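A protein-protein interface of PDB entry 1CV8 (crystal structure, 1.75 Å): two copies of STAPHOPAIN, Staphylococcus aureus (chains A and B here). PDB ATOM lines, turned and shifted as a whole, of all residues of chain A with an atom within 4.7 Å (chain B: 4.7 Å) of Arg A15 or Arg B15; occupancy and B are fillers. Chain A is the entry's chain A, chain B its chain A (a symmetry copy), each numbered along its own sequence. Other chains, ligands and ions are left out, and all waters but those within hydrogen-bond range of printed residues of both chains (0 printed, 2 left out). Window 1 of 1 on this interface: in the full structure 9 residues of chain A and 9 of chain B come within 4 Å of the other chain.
The backbone carbonyl oxygen (O) of Ile B14 sits at hydrogen-bond distance from the side-chain amino group (NZ) of Lys A13, at 3.1 Å. NZ of Lys B13 is in hydrogen-bond range of O of Ile A14 (3.1 Å).
Arg B15 touches Arg A15. Arg A15 touches Asn B40 (O to CB, 3.7 Å). Asn B40 touches Glu A16 (CG to CA, 3.6 Å). Arg B15 touches Asn A40. Asn A40 touches Glu B16 (CG to CA, 3.6 Å).
Of the printed residues of chain B, Arg A15 touches Arg B15 (3.2 Å) and Asn B40 (3.7 Å). Arg B15 touches just these residues of chain A: Arg A15 (3.2 Å) and Asn A40 (3.7 Å). Of the printed residues of chain A, Glu B16 touches Asn A40 (3.6 Å). Of the printed residues of chain B, Glu A16 touches Asn B40. Printed residues of chain B within 4 Å of Ile A14: Lys B13 (3.1 Å). Thr B39 touches none of the printed residues of chain A. The nearest residue of chain B that does not touch Arg A15 is Lys B13 (4.3 Å). The nearest printed residue of chain B that does not touch Lys A13 is Lys B13 (4.3 Å).
Along chain A the printed residues that touch a printed residue of chain B span positions 13 to 40. Among the printed residues, 7 pairs touch across the chains. Among the printed residues, no Asp or Glu carboxylate lies within 4 Å of a Lys or Arg side-chain nitrogen of the other chain.
Lys A13 touches Ile B14, and with the chains exchanged Ile A14 touches Lys B13. Arg B15 touches its own counterpart, Arg A15. Arg A15 touches Asn B40, and with the chains exchanged Asn A40 touches Arg B15. Glu A16 touches Asn B40, and with the chains exchanged Asn A40 touches Glu B16. 7 positions are printed for both chains. Of the 7 pairs that touch across the chains among the printed residues, 7 have their exchanged pair printed and touching as well.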
ATOM      1  N   LYS A  13     -20.194  28.611  -1.788  1.00  0.00           N
ATOM      2  CA  LYS A  13     -21.252  27.701  -2.189  1.00  0.00           C
ATOM      3  C   LYS A  13     -21.410  27.687  -3.672  1.00  0.00           C
ATOM      4  O   LYS A  13     -21.395  28.756  -4.266  1.00  0.00           O
ATOM      5  CB  LYS A  13     -22.574  28.224  -1.525  1.00  0.00           C
ATOM      6  CG  LYS A  13     -23.801  27.400  -1.841  1.00  0.00           C
ATOM      7  CD  LYS A  13     -24.979  27.919  -0.980  1.00  0.00           C
ATOM      8  CE  LYS A  13     -26.215  27.071  -1.182  1.00  0.00           C
ATOM      9  NZ  LYS A  13     -27.435  27.856  -1.574  1.00  0.00           N
ATOM     10  N   ILE A  14     -21.537  26.516  -4.369  1.00  0.00           N
ATOM     11  CA  ILE A  14     -21.837  26.552  -5.782  1.00  0.00           C
ATOM     12  C   ILE A  14     -23.338  26.802  -5.975  1.00  0.00           C
ATOM     13  O   ILE A  14     -24.113  26.028  -5.372  1.00  0.00           O
ATOM     14  CB  ILE A  14     -21.499  25.139  -6.408  1.00  0.00           C
ATOM     15  CG1 ILE A  14     -20.007  24.882  -6.107  1.00  0.00           C
ATOM     16  CG2 ILE A  14     -21.801  25.131  -7.895  1.00  0.00           C
ATOM     17  CD1 ILE A  14     -19.630  23.414  -6.467  1.00  0.00           C
ATOM     18  N   ARG A  15     -23.680  27.832  -6.683  1.00  0.00           N
ATOM     19  CA  ARG A  15     -25.098  28.153  -6.922  1.00  0.00           C
ATOM     20  C   ARG A  15     -25.489  28.090  -8.375  1.00  0.00           C
ATOM     21  O   ARG A  15     -26.670  28.200  -8.803  1.00  0.00           O
ATOM     22  CB  ARG A  15     -25.317  29.611  -6.377  1.00  0.00           C
ATOM     23  CG  ARG A  15     -25.346  29.678  -4.854  1.00  0.00           C
ATOM     24  CD  ARG A  15     -25.653  31.164  -4.463  1.00  0.00           C
ATOM     25  NE  ARG A  15     -25.646  31.251  -2.987  1.00  0.00           N
ATOM     26  CZ  ARG A  15     -24.620  31.544  -2.219  1.00  0.00           C
ATOM     27  NH1 ARG A  15     -23.410  31.776  -2.797  1.00  0.00           N
ATOM     28  NH2 ARG A  15     -24.775  31.619  -0.887  1.00  0.00           N
ATOM     29  N   GLU A  16     -24.462  27.955  -9.309  1.00  0.00           N
ATOM     30  CA  GLU A  16     -24.827  27.853 -10.725  1.00  0.00           C
ATOM     31  C   GLU A  16     -23.584  27.197 -11.448  1.00  0.00           C
ATOM     32  O   GLU A  16     -22.516  27.299 -10.874  1.00  0.00           O
ATOM     33  CB  GLU A  16     -25.079  29.165 -11.448  1.00  0.00           C
ATOM     34  CG  GLU A  16     -24.131  30.275 -10.968  1.00  0.00           C
ATOM     35  CD  GLU A  16     -24.293  31.631 -11.567  1.00  0.00           C
ATOM     36  OE1 GLU A  16     -25.273  31.910 -12.275  1.00  0.00           O
ATOM     37  OE2 GLU A  16     -23.355  32.465 -11.433  1.00  0.00           O
ATOM     38  N   ASN A  34     -19.631  36.276  -3.648  1.00  0.00           N
ATOM     39  CA  ASN A  34     -20.704  35.761  -2.749  1.00  0.00           C
ATOM     40  C   ASN A  34     -20.122  35.223  -1.460  1.00  0.00           C
ATOM     41  O   ASN A  34     -20.645  35.320  -0.341  1.00  0.00           O
ATOM     42  CB  ASN A  34     -21.561  34.733  -3.473  1.00  0.00           C
ATOM     43  CG  ASN A  34     -22.549  35.289  -4.432  1.00  0.00           C
ATOM     44  OD1 ASN A  34     -22.968  36.463  -4.338  1.00  0.00           O
ATOM     45  ND2 ASN A  34     -23.015  34.463  -5.401  1.00  0.00           N
ATOM     46  N   THR A  39     -23.017  36.588   0.768  1.00  0.00           N
ATOM     47  CA  THR A  39     -24.212  36.997   0.101  1.00  0.00           C
ATOM     48  C   THR A  39     -24.501  35.975  -1.028  1.00  0.00           C
ATOM     49  O   THR A  39     -23.731  35.025  -1.189  1.00  0.00           O
ATOM     50  CB  THR A  39     -24.163  38.452  -0.404  1.00  0.00           C
ATOM     51  OG1 THR A  39     -25.407  38.845  -0.982  1.00  0.00           O
ATOM     52  CG2 THR A  39     -23.051  38.590  -1.469  1.00  0.00           C
ATOM     53  N   ASN A  40     -25.598  36.114  -1.693  1.00  0.00           N
ATOM     54  CA  ASN A  40     -26.048  35.313  -2.819  1.00  0.00           C
ATOM     55  C   ASN A  40     -26.437  36.190  -3.972  1.00  0.00           C
ATOM     56  O   ASN A  40     -26.996  35.690  -4.974  1.00  0.00           O
ATOM     57  CB  ASN A  40     -27.120  34.337  -2.356  1.00  0.00           C
ATOM     58  CG  ASN A  40     -28.325  35.149  -1.740  1.00  0.00           C
ATOM     59  OD1 ASN A  40     -28.698  36.134  -2.319  1.00  0.00           O
ATOM     60  ND2 ASN A  40     -28.802  34.538  -0.684  1.00  0.00           N
ATOM     61  N   LYS B  13     -34.210  24.063  -4.560  1.00  0.00           N
ATOM     62  CA  LYS B  13     -33.096  24.568  -3.776  1.00  0.00           C
ATOM     63  C   LYS B  13     -33.143  26.055  -3.679  1.00  0.00           C
ATOM     64  O   LYS B  13     -33.394  26.694  -4.692  1.00  0.00           O
ATOM     65  CB  LYS B  13     -31.786  24.129  -4.522  1.00  0.00           C
ATOM     66  CG  LYS B  13     -30.508  24.579  -3.852  1.00  0.00           C
ATOM     67  CD  LYS B  13     -29.311  23.927  -4.587  1.00  0.00           C
ATOM     68  CE  LYS B  13     -28.005  24.262  -3.904  1.00  0.00           C
ATOM     69  NZ  LYS B  13     -26.976  24.867  -4.820  1.00  0.00           N
ATOM     70  N   ILE B  14     -32.943  26.702  -2.491  1.00  0.00           N
ATOM     71  CA  ILE B  14     -32.848  28.144  -2.466  1.00  0.00           C
ATOM     72  C   ILE B  14     -31.439  28.566  -2.906  1.00  0.00           C
ATOM     73  O   ILE B  14     -30.485  28.044  -2.290  1.00  0.00           O
ATOM     74  CB  ILE B  14     -33.059  28.641  -0.981  1.00  0.00           C
ATOM     75  CG1 ILE B  14     -34.442  28.114  -0.543  1.00  0.00           C
ATOM     76  CG2 ILE B  14     -32.965  30.155  -0.908  1.00  0.00           C
ATOM     77  CD1 ILE B  14     -34.648  28.341   0.985  1.00  0.00           C
ATOM     78  N   ARG B  15     -31.351  29.367  -3.920  1.00  0.00           N
ATOM     79  CA  ARG B  15     -30.042  29.826  -4.414  1.00  0.00           C
ATOM     80  C   ARG B  15     -29.849  31.316  -4.302  1.00  0.00           C
ATOM     81  O   ARG B  15     -28.766  31.916  -4.542  1.00  0.00           O
ATOM     82  CB  ARG B  15     -29.966  29.394  -5.924  1.00  0.00           C
ATOM     83  CG  ARG B  15     -29.738  27.896  -6.101  1.00  0.00           C
ATOM     84  CD  ARG B  15     -29.599  27.630  -7.640  1.00  0.00           C
ATOM     85  NE  ARG B  15     -29.417  26.176  -7.829  1.00  0.00           N
ATOM     86  CZ  ARG B  15     -30.360  25.282  -8.033  1.00  0.00           C
ATOM     87  NH1 ARG B  15     -31.658  25.688  -8.055  1.00  0.00           N
ATOM     88  NH2 ARG B  15     -30.036  23.991  -8.222  1.00  0.00           N
ATOM     89  N   GLU B  16     -30.962  32.082  -3.962  1.00  0.00           N
ATOM     90  CA  GLU B  16     -30.784  33.529  -3.812  1.00  0.00           C
ATOM     91  C   GLU B  16     -32.005  34.029  -2.942  1.00  0.00           C
ATOM     92  O   GLU B  16     -32.989  33.312  -2.937  1.00  0.00           O
ATOM     93  CB  GLU B  16     -30.828  34.347  -5.091  1.00  0.00           C
ATOM     94  CG  GLU B  16     -31.852  33.791  -6.092  1.00  0.00           C
ATOM     95  CD  GLU B  16     -31.973  34.475  -7.411  1.00  0.00           C
ATOM     96  OE1 GLU B  16     -31.150  35.331  -7.771  1.00  0.00           O
ATOM     97  OE2 GLU B  16     -32.995  34.248  -8.117  1.00  0.00           O
ATOM     98  N   ASN B  34     -36.133  26.208 -11.923  1.00  0.00           N
ATOM     99  CA  ASN B  34     -34.884  25.448 -11.625  1.00  0.00           C
ATOM    100  C   ASN B  34     -35.200  24.063 -11.105  1.00  0.00           C
ATOM    101  O   ASN B  34     -34.548  23.039 -11.352  1.00  0.00           O
ATOM    102  CB  ASN B  34     -33.993  26.236 -10.676  1.00  0.00           C
ATOM    103  CG  ASN B  34     -33.237  27.356 -11.292  1.00  0.00           C
ATOM    104  OD1 ASN B  34     -32.985  27.384 -12.517  1.00  0.00           O
ATOM    105  ND2 ASN B  34     -32.793  28.340 -10.471  1.00  0.00           N
ATOM    106  N   THR B  39     -32.255  22.353 -13.009  1.00  0.00           N
ATOM    107  CA  THR B  39     -31.236  23.206 -13.528  1.00  0.00           C
ATOM    108  C   THR B  39     -30.958  24.312 -12.479  1.00  0.00           C
ATOM    109  O   THR B  39     -31.596  24.311 -11.422  1.00  0.00           O
ATOM    110  CB  THR B  39     -31.566  23.773 -14.923  1.00  0.00           C
ATOM    111  OG1 THR B  39     -30.482  24.544 -15.441  1.00  0.00           O
ATOM    112  CG2 THR B  39     -32.820  24.669 -14.833  1.00  0.00           C
ATOM    113  N   ASN B  40     -29.995  25.136 -12.720  1.00  0.00           N
ATOM    114  CA  ASN B  40     -29.592  26.274 -11.910  1.00  0.00           C
ATOM    115  C   ASN B  40     -29.496  27.514 -12.748  1.00  0.00           C
ATOM    116  O   ASN B  40     -29.013  28.561 -12.258  1.00  0.00           O
ATOM    117  CB  ASN B  40     -28.336  25.923 -11.124  1.00  0.00           C
ATOM    118  CG  ASN B  40     -27.189  25.530 -12.134  1.00  0.00           C
ATOM    119  OD1 ASN B  40     -27.046  26.208 -13.118  1.00  0.00           O
ATOM    120  ND2 ASN B  40     -26.488  24.526 -11.671  1.00  0.00           N
